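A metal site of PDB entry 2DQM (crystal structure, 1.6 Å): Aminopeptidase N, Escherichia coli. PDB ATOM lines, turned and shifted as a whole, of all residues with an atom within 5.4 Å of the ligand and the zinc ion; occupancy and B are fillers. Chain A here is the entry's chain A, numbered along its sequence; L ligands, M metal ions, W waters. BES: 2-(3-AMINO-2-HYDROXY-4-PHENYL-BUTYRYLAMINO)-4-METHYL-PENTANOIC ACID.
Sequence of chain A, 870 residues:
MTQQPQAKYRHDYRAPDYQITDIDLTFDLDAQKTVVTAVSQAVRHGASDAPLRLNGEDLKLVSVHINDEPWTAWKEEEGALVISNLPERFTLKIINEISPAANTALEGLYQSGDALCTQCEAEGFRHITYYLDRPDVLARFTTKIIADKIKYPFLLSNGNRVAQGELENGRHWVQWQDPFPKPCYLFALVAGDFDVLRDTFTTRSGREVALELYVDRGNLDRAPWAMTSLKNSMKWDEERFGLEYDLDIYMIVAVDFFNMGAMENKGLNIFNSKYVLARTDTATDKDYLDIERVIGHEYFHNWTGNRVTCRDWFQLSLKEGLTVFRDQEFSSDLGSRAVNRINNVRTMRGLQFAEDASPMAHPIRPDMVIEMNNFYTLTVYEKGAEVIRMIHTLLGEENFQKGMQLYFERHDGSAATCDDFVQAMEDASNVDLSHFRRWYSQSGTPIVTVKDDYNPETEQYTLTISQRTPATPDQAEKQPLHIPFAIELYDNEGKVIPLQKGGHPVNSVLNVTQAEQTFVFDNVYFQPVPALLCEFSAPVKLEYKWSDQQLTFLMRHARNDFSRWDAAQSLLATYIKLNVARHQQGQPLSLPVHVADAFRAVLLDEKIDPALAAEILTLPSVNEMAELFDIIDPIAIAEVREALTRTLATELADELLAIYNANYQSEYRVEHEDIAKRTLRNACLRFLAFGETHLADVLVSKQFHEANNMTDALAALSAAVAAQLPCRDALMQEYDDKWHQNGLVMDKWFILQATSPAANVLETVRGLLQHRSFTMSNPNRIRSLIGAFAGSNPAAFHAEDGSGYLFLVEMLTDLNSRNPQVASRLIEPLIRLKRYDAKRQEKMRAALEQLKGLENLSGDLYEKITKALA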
ATOM      1  N   GLN A 119      31.613  -3.693   2.642  1.00  0.00           N
ATOM      2  CA  GLN A 119      30.846  -4.755   2.009  1.00  0.00           C
ATOM      3  C   GLN A 119      31.698  -5.977   2.308  1.00  0.00           C
ATOM      4  O   GLN A 119      32.785  -6.125   1.741  1.00  0.00           O
ATOM      5  CB  GLN A 119      30.679  -4.566   0.503  1.00  0.00           C
ATOM      6  CG  GLN A 119      29.922  -5.739  -0.150  1.00  0.00           C
ATOM      7  CD  GLN A 119      28.663  -6.146   0.612  1.00  0.00           C
ATOM      8  OE1 GLN A 119      27.904  -5.290   1.091  1.00  0.00           O
ATOM      9  NE2 GLN A 119      28.421  -7.444   0.728  1.00  0.00           N
ATOM     10  N   GLU A 121      30.318  -9.558   2.534  1.00  0.00           N
ATOM     11  CA  GLU A 121      29.865 -10.820   1.960  1.00  0.00           C
ATOM     12  C   GLU A 121      30.196 -10.886   0.471  1.00  0.00           C
ATOM     13  O   GLU A 121      30.076  -9.920  -0.254  1.00  0.00           O
ATOM     14  CB  GLU A 121      28.362 -10.989   2.171  1.00  0.00           C
ATOM     15  CG  GLU A 121      27.801 -12.290   1.643  1.00  0.00           C
ATOM     16  CD  GLU A 121      26.283 -12.344   1.693  1.00  0.00           C
ATOM     17  OE1 GLU A 121      25.717 -13.431   1.409  1.00  0.00           O
ATOM     18  OE2 GLU A 121      25.667 -11.317   2.015  1.00  0.00           O
ATOM     19  N   ALA A 122      30.708 -12.030  -0.012  1.00  0.00           N
ATOM     20  CA  ALA A 122      30.886 -13.272   0.747  1.00  0.00           C
ATOM     21  C   ALA A 122      32.165 -13.220   1.583  1.00  0.00           C
ATOM     22  O   ALA A 122      31.989 -13.567   2.765  1.00  0.00           O
ATOM     23  CB  ALA A 122      30.934 -14.457  -0.208  1.00  0.00           C
ATOM     24  N   MET A 260      26.075  -4.329  -5.540  1.00  0.00           N
ATOM     25  CA  MET A 260      24.800  -5.024  -5.618  1.00  0.00           C
ATOM     26  C   MET A 260      23.661  -4.078  -5.261  1.00  0.00           C
ATOM     27  O   MET A 260      23.756  -2.863  -5.469  1.00  0.00           O
ATOM     28  CB  MET A 260      24.794  -6.259  -4.709  1.00  0.00           C
ATOM     29  CG  MET A 260      25.291  -6.020  -3.295  1.00  0.00           C
ATOM     30  SD  MET A 260      27.044  -5.588  -3.209  1.00  0.00           S
ATOM     31  CE  MET A 260      27.808  -7.192  -3.344  1.00  0.00           C
ATOM     32  N   GLY A 261      22.573  -4.636  -4.736  1.00  0.00           N
ATOM     33  CA  GLY A 261      21.430  -3.827  -4.377  1.00  0.00           C
ATOM     34  C   GLY A 261      21.390  -3.427  -2.915  1.00  0.00           C
ATOM     35  O   GLY A 261      21.131  -2.275  -2.591  1.00  0.00           O
ATOM     36  N   ALA A 262      21.638  -4.384  -2.024  1.00  0.00           N
ATOM     37  CA  ALA A 262      21.619  -4.100  -0.590  1.00  0.00           C
ATOM     38  C   ALA A 262      22.296  -5.223   0.189  1.00  0.00           C
ATOM     39  O   ALA A 262      22.560  -6.290  -0.361  1.00  0.00           O
ATOM     40  CB  ALA A 262      20.170  -3.929  -0.123  1.00  0.00           C
ATOM     41  N   MET A 263      22.565  -4.980   1.474  1.00  0.00           N
ATOM     42  CA  MET A 263      23.246  -5.957   2.326  1.00  0.00           C
ATOM     43  C   MET A 263      22.659  -5.956   3.739  1.00  0.00           C
ATOM     44  O   MET A 263      22.527  -4.899   4.366  1.00  0.00           O
ATOM     45  CB  MET A 263      24.739  -5.638   2.356  1.00  0.00           C
ATOM     46  CG  MET A 263      25.567  -6.587   3.204  1.00  0.00           C
ATOM     47  SD  MET A 263      25.460  -8.290   2.607  1.00  0.00           S
ATOM     48  CE  MET A 263      25.505  -9.173   4.177  1.00  0.00           C
ATOM     49  N   GLU A 264      22.360  -7.141   4.234  1.00  0.00           N
ATOM     50  CA  GLU A 264      21.729  -7.320   5.543  1.00  0.00           C
ATOM     51  C   GLU A 264      22.599  -7.267   6.813  1.00  0.00           C
ATOM     52  O   GLU A 264      22.269  -7.924   7.802  1.00  0.00           O
ATOM     53  CB  GLU A 264      20.946  -8.642   5.541  1.00  0.00           C
ATOM     54  CG  GLU A 264      21.806  -9.927   5.596  1.00  0.00           C
ATOM     55  CD  GLU A 264      22.282 -10.431   4.238  1.00  0.00           C
ATOM     56  OE1 GLU A 264      22.671 -11.623   4.155  1.00  0.00           O
ATOM     57  OE2 GLU A 264      22.282  -9.659   3.252  1.00  0.00           O
ATOM     58  N   ARG A 293      10.381  -4.127  -1.873  1.00  0.00           N
ATOM     59  CA  ARG A 293      10.897  -5.487  -1.922  1.00  0.00           C
ATOM     60  C   ARG A 293      12.273  -5.649  -1.294  1.00  0.00           C
ATOM     61  O   ARG A 293      12.485  -6.567  -0.511  1.00  0.00           O
ATOM     62  CB  ARG A 293      10.980  -5.987  -3.372  1.00  0.00           C
ATOM     63  CG  ARG A 293      11.554  -7.390  -3.435  1.00  0.00           C
ATOM     64  CD  ARG A 293      11.935  -7.867  -4.825  1.00  0.00           C
ATOM     65  NE  ARG A 293      12.494  -9.209  -4.720  1.00  0.00           N
ATOM     66  CZ  ARG A 293      13.545  -9.663  -5.403  1.00  0.00           C
ATOM     67  NH1 ARG A 293      14.172  -8.874  -6.268  1.00  0.00           N
ATOM     68  NH2 ARG A 293      13.971 -10.900  -5.187  1.00  0.00           N
ATOM     69  N   VAL A 294      13.191  -4.768  -1.652  1.00  0.00           N
ATOM     70  CA  VAL A 294      14.565  -4.856  -1.147  1.00  0.00           C
ATOM     71  C   VAL A 294      14.667  -4.491   0.338  1.00  0.00           C
ATOM     72  O   VAL A 294      15.389  -5.150   1.088  1.00  0.00           O
ATOM     73  CB  VAL A 294      15.520  -3.971  -1.983  1.00  0.00           C
ATOM     74  CG1 VAL A 294      16.945  -4.106  -1.473  1.00  0.00           C
ATOM     75  CG2 VAL A 294      15.451  -4.401  -3.451  1.00  0.00           C
ATOM     76  N   HIS A 297      13.319  -7.526   1.971  1.00  0.00           N
ATOM     77  CA  HIS A 297      14.265  -8.634   1.812  1.00  0.00           C
ATOM     78  C   HIS A 297      15.395  -8.604   2.855  1.00  0.00           C
ATOM     79  O   HIS A 297      15.605  -9.576   3.573  1.00  0.00           O
ATOM     80  CB  HIS A 297      14.875  -8.593   0.415  1.00  0.00           C
ATOM     81  CG  HIS A 297      15.817  -9.720   0.123  1.00  0.00           C
ATOM     82  ND1 HIS A 297      15.420 -10.869  -0.528  1.00  0.00           N
ATOM     83  CD2 HIS A 297      17.124  -9.890   0.411  1.00  0.00           C
ATOM     84  CE1 HIS A 297      16.448 -11.689  -0.646  1.00  0.00           C
ATOM     85  NE2 HIS A 297      17.500 -11.110  -0.074  1.00  0.00           N
ATOM     86  N   GLU A 298      16.119  -7.486   2.925  1.00  0.00           N
ATOM     87  CA  GLU A 298      17.223  -7.406   3.875  1.00  0.00           C
ATOM     88  C   GLU A 298      16.699  -7.497   5.308  1.00  0.00           C
ATOM     89  O   GLU A 298      17.372  -8.079   6.166  1.00  0.00           O
ATOM     90  CB  GLU A 298      18.022  -6.116   3.674  1.00  0.00           C
ATOM     91  CG  GLU A 298      18.540  -5.867   2.240  1.00  0.00           C
ATOM     92  CD  GLU A 298      19.161  -7.090   1.571  1.00  0.00           C
ATOM     93  OE1 GLU A 298      19.707  -7.964   2.268  1.00  0.00           O
ATOM     94  OE2 GLU A 298      19.127  -7.145   0.318  1.00  0.00           O
ATOM     95  N   HIS A 301      16.152 -11.044   6.333  1.00  0.00           N
ATOM     96  CA  HIS A 301      17.396 -11.763   6.595  1.00  0.00           C
ATOM     97  C   HIS A 301      17.739 -11.731   8.081  1.00  0.00           C
ATOM     98  O   HIS A 301      18.517 -12.552   8.559  1.00  0.00           O
ATOM     99  CB  HIS A 301      18.571 -11.134   5.845  1.00  0.00           C
ATOM    100  CG  HIS A 301      18.840 -11.745   4.500  1.00  0.00           C
ATOM    101  ND1 HIS A 301      18.971 -13.098   4.309  1.00  0.00           N
ATOM    102  CD2 HIS A 301      19.043 -11.161   3.300  1.00  0.00           C
ATOM    103  CE1 HIS A 301      19.242 -13.340   3.042  1.00  0.00           C
ATOM    104  NE2 HIS A 301      19.289 -12.181   2.406  1.00  0.00           N
ATOM    105  N   LYS A 319      19.771 -19.135   2.944  1.00  0.00           N
ATOM    106  CA  LYS A 319      19.284 -17.811   3.323  1.00  0.00           C
ATOM    107  C   LYS A 319      18.717 -17.029   2.134  1.00  0.00           C
ATOM    108  O   LYS A 319      17.703 -16.355   2.268  1.00  0.00           O
ATOM    109  CB  LYS A 319      20.373 -16.996   4.041  1.00  0.00           C
ATOM    110  CG  LYS A 319      21.552 -16.489   3.213  1.00  0.00           C
ATOM    111  CD  LYS A 319      22.502 -15.688   4.131  1.00  0.00           C
ATOM    112  CE  LYS A 319      23.739 -15.133   3.425  1.00  0.00           C
ATOM    113  NZ  LYS A 319      23.463 -13.917   2.601  1.00  0.00           N
ATOM    114  N   GLU A 320      19.344 -17.122   0.969  1.00  0.00           N
ATOM    115  CA  GLU A 320      18.838 -16.358  -0.175  1.00  0.00           C
ATOM    116  C   GLU A 320      17.546 -16.892  -0.786  1.00  0.00           C
ATOM    117  O   GLU A 320      16.645 -16.113  -1.096  1.00  0.00           O
ATOM    118  CB  GLU A 320      19.927 -16.231  -1.257  1.00  0.00           C
ATOM    119  CG  GLU A 320      21.167 -15.446  -0.821  1.00  0.00           C
ATOM    120  CD  GLU A 320      20.835 -14.091  -0.221  1.00  0.00           C
ATOM    121  OE1 GLU A 320      19.754 -13.554  -0.516  1.00  0.00           O
ATOM    122  OE2 GLU A 320      21.675 -13.559   0.546  1.00  0.00           O
ATOM    123  N   THR A 323      14.857 -16.226   1.825  1.00  0.00           N
ATOM    124  CA  THR A 323      14.569 -14.810   1.994  1.00  0.00           C
ATOM    125  C   THR A 323      13.898 -14.223   0.755  1.00  0.00           C
ATOM    126  O   THR A 323      13.110 -13.288   0.871  1.00  0.00           O
ATOM    127  CB  THR A 323      15.834 -14.033   2.372  1.00  0.00           C
ATOM    128  OG1 THR A 323      16.343 -14.575   3.605  1.00  0.00           O
ATOM    129  CG2 THR A 323      15.531 -12.554   2.582  1.00  0.00           C
ATOM    130  N   VAL A 324      14.212 -14.766  -0.424  1.00  0.00           N
ATOM    131  CA  VAL A 324      13.549 -14.286  -1.630  1.00  0.00           C
ATOM    132  C   VAL A 324      12.092 -14.746  -1.541  1.00  0.00           C
ATOM    133  O   VAL A 324      11.173 -14.005  -1.885  1.00  0.00           O
ATOM    134  CB  VAL A 324      14.198 -14.875  -2.913  1.00  0.00           C
ATOM    135  CG1 VAL A 324      13.253 -14.673  -4.109  1.00  0.00           C
ATOM    136  CG2 VAL A 324      15.527 -14.188  -3.194  1.00  0.00           C
ATOM    137  N   ASP A 327      10.453 -12.330   0.644  1.00  0.00           N
ATOM    138  CA  ASP A 327      10.169 -11.021   0.059  1.00  0.00           C
ATOM    139  C   ASP A 327       9.056 -11.108  -0.980  1.00  0.00           C
ATOM    140  O   ASP A 327       8.311 -10.144  -1.164  1.00  0.00           O
ATOM    141  CB  ASP A 327      11.447 -10.315  -0.476  1.00  0.00           C
ATOM    142  CG  ASP A 327      11.892 -10.754  -1.882  1.00  0.00           C
ATOM    143  OD1 ASP A 327      11.073 -10.760  -2.831  1.00  0.00           O
ATOM    144  OD2 ASP A 327      13.101 -11.037  -2.049  1.00  0.00           O
ATOM    145  N   ASN A 373      31.675 -14.891  -5.370  1.00  0.00           N
ATOM    146  CA  ASN A 373      30.869 -13.754  -5.812  1.00  0.00           C
ATOM    147  C   ASN A 373      30.153 -14.044  -7.129  1.00  0.00           C
ATOM    148  O   ASN A 373      29.265 -13.291  -7.526  1.00  0.00           O
ATOM    149  CB  ASN A 373      31.714 -12.478  -5.918  1.00  0.00           C
ATOM    150  CG  ASN A 373      32.007 -11.857  -4.558  1.00  0.00           C
ATOM    151  OD1 ASN A 373      31.149 -11.841  -3.677  1.00  0.00           O
ATOM    152  ND2 ASN A 373      33.219 -11.341  -4.398  1.00  0.00           N
ATOM    153  N   TYR A 376      25.869 -15.550  -6.693  1.00  0.00           N
ATOM    154  CA  TYR A 376      24.686 -14.843  -6.187  1.00  0.00           C
ATOM    155  C   TYR A 376      23.854 -14.734  -7.454  1.00  0.00           C
ATOM    156  O   TYR A 376      23.641 -13.660  -8.025  1.00  0.00           O
ATOM    157  CB  TYR A 376      25.095 -13.494  -5.597  1.00  0.00           C
ATOM    158  CG  TYR A 376      25.777 -13.687  -4.262  1.00  0.00           C
ATOM    159  CD1 TYR A 376      27.081 -14.180  -4.180  1.00  0.00           C
ATOM    160  CD2 TYR A 376      25.074 -13.466  -3.082  1.00  0.00           C
ATOM    161  CE1 TYR A 376      27.668 -14.442  -2.940  1.00  0.00           C
ATOM    162  CE2 TYR A 376      25.647 -13.729  -1.846  1.00  0.00           C
ATOM    163  CZ  TYR A 376      26.941 -14.221  -1.777  1.00  0.00           C
ATOM    164  OH  TYR A 376      27.505 -14.496  -0.557  1.00  0.00           O
ATOM    165  N   TYR A 381      19.018 -17.723  -6.032  1.00  0.00           N
ATOM    166  CA  TYR A 381      17.951 -16.848  -5.564  1.00  0.00           C
ATOM    167  C   TYR A 381      16.556 -17.240  -6.016  1.00  0.00           C
ATOM    168  O   TYR A 381      15.751 -17.710  -5.210  1.00  0.00           O
ATOM    169  CB  TYR A 381      18.211 -15.403  -6.005  1.00  0.00           C
ATOM    170  CG  TYR A 381      19.205 -14.649  -5.158  1.00  0.00           C
ATOM    171  CD1 TYR A 381      20.538 -15.053  -5.081  1.00  0.00           C
ATOM    172  CD2 TYR A 381      18.798 -13.527  -4.427  1.00  0.00           C
ATOM    173  CE1 TYR A 381      21.437 -14.349  -4.282  1.00  0.00           C
ATOM    174  CE2 TYR A 381      19.687 -12.835  -3.644  1.00  0.00           C
ATOM    175  CZ  TYR A 381      21.014 -13.246  -3.570  1.00  0.00           C
ATOM    176  OH  TYR A 381      21.896 -12.548  -2.788  1.00  0.00           O
ATOM    177  N   GLN A 821      33.800  -7.778  -9.836  1.00  0.00           N
ATOM    178  CA  GLN A 821      32.416  -8.177  -9.650  1.00  0.00           C
ATOM    179  C   GLN A 821      31.486  -7.602 -10.711  1.00  0.00           C
ATOM    180  O   GLN A 821      30.634  -8.315 -11.243  1.00  0.00           O
ATOM    181  CB  GLN A 821      31.924  -7.776  -8.254  1.00  0.00           C
ATOM    182  CG  GLN A 821      32.529  -8.599  -7.136  1.00  0.00           C
ATOM    183  CD  GLN A 821      31.967  -8.218  -5.776  1.00  0.00           C
ATOM    184  OE1 GLN A 821      30.775  -8.384  -5.517  1.00  0.00           O
ATOM    185  NE2 GLN A 821      32.831  -7.710  -4.911  1.00  0.00           N
HETATM  186  N2  BES L   1      23.096 -10.866   0.932  1.00  0.00           N
HETATM  187  C1  BES L   1      22.781 -10.125  -0.309  1.00  0.00           C
HETATM  188  C6  BES L   1      23.886  -9.090  -0.593  1.00  0.00           C
HETATM  189  C7  BES L   1      24.943  -9.611  -1.542  1.00  0.00           C
HETATM  190  C8  BES L   1      24.692  -9.681  -2.935  1.00  0.00           C
HETATM  191  C12 BES L   1      26.203 -10.019  -1.041  1.00  0.00           C
HETATM  192  C9  BES L   1      25.699 -10.160  -3.816  1.00  0.00           C
HETATM  193  C11 BES L   1      27.206 -10.500  -1.913  1.00  0.00           C
HETATM  194  C10 BES L   1      26.948 -10.564  -3.306  1.00  0.00           C
HETATM  195  C2  BES L   1      21.430  -9.392  -0.186  1.00  0.00           C
HETATM  196  O2  BES L   1      20.647  -9.929   0.878  1.00  0.00           O
HETATM  197  C3  BES L   1      20.683  -9.521  -1.489  1.00  0.00           C
HETATM  198  O3  BES L   1      20.338 -10.628  -1.872  1.00  0.00           O
HETATM  199  N1  BES L   1      20.511  -8.422  -2.255  1.00  0.00           N
HETATM  200  C4  BES L   1      19.958  -8.436  -3.627  1.00  0.00           C
HETATM  201  C13 BES L   1      18.544  -7.806  -3.681  1.00  0.00           C
HETATM  202  C14 BES L   1      17.503  -8.629  -2.911  1.00  0.00           C
HETATM  203  C15 BES L   1      16.168  -7.895  -2.941  1.00  0.00           C
HETATM  204  C16 BES L   1      17.320  -9.993  -3.587  1.00  0.00           C
HETATM  205  C5  BES L   1      20.914  -7.624  -4.456  1.00  0.00           C
HETATM  206  O1  BES L   1      21.842  -6.862  -3.839  1.00  0.00           O
HETATM  207  O4  BES L   1      20.859  -7.652  -5.667  1.00  0.00           O
HETATM  208 ZN    ZN M   1      19.465 -11.718   0.356  1.00  0.00          ZN
HETATM  209  O   HOH W   1      22.124 -10.580  -6.728  1.00  0.00           O
HETATM  210  O   HOH W   2      22.169  -6.343  -7.702  1.00  0.00           O
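OE2 of Glu 320 is in salt-bridge range of NZ of Lys 319 (2.7 Å).
N of Glu 264 lies within hydrogen-bond range of OE1 of Glu 298 (3.4 Å).
A ring nitrogen (ND1) of His 297 lies within hydrogen-bond range of the side-chain carboxylate (OD2) of Asp 327, at 2.8 Å.
The guanidinium group of Arg 293 lies within salt-bridge range of the side-chain carboxylate of Asp 327, 2.8 Å away.
A ring nitrogen (ND1) of His 301 sits at hydrogen-bond distance from the side-chain hydroxyl of Thr 323, 3.1 Å away.
The side-chain carboxylate (OE1) of Glu 264 is in salt-bridge range of the side-chain amino group (NZ) of Lys 319 (2.9 Å).
The backbone carbonyl oxygen (O) of Glu 121 lies within hydrogen-bond range of the side-chain amide nitrogen (NE2) of Gln 119 (3.1 Å).
The side-chain sulfur of Met 263 sits at hydrogen-bond distance from the side-chain amide nitrogen of Gln 119, at 3.6 Å.
The backbone NH (N) of Ala 262 is in hydrogen-bond range of an oxygen (O1) of the ligand, at 3.1 Å.
An oxygen (O3) of the ligand sits at hydrogen-bond distance from the side-chain hydroxyl (OH) of Tyr 381 (2.6 Å).
The side-chain amino group (NZ) of Lys 319 sits close to a nitrogen (N2) of the ligand.
The side-chain carboxylate (OE2) of Glu 264 is in salt-bridge range of a nitrogen (N2) of the ligand (2.7 Å).
The side-chain carboxylate (OE2) of Glu 298 is in hydrogen-bond range of a nitrogen (N1) of the ligand.
The backbone NH of Gly 261 lies within hydrogen-bond range of an oxygen (O1) of the ligand, 2.5 Å away.
The side-chain carboxylate (OE2) of Glu 121 lies within salt-bridge range of a nitrogen (N2) of the ligand (2.8 Å).
Residues that only touch the ligand: Gln 119 (3.8 Å), Met 260 (3.1 Å), Met 263 (3.7 Å), Arg 293 (3.8 Å), Val 294 (3.6 Å) and Tyr 376 (3.4 Å).
Hydrophobic or aromatic side chains that line the ligand: Met 260, Met 263, Val 294, His 297, His 301, Tyr 376 and Tyr 381.
16 residues have an atom within 4 Å of the ligand: Gln 119, Glu 121, Met 260, Gly 261, Ala 262, Met 263, Glu 264, Arg 293, Val 294, His 297, Glu 298, His 301, Lys 319, Glu 320, Tyr 376 and Tyr 381.
The nearest printed residue that does not touch the ligand is Ala 122 (4.3 Å).
Within 4 Å of the zinc ion: His 297, His 301 and Glu 320.
Water W2 lies within hydrogen-bond range of an oxygen (O4) of the ligand (2.8 Å) and the backbone NH of Gly 261 (3.4 Å).
The zinc ion is bound by OE1 of Glu 320 (2.1 Å), NE2 of His 297 (2.1 Å), NE2 of His 301 (2.1 Å) and O2 of the ligand (2.2 Å).
Slightly farther from the zinc ion lies an oxygen (O3) of the ligand (2.6 Å).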
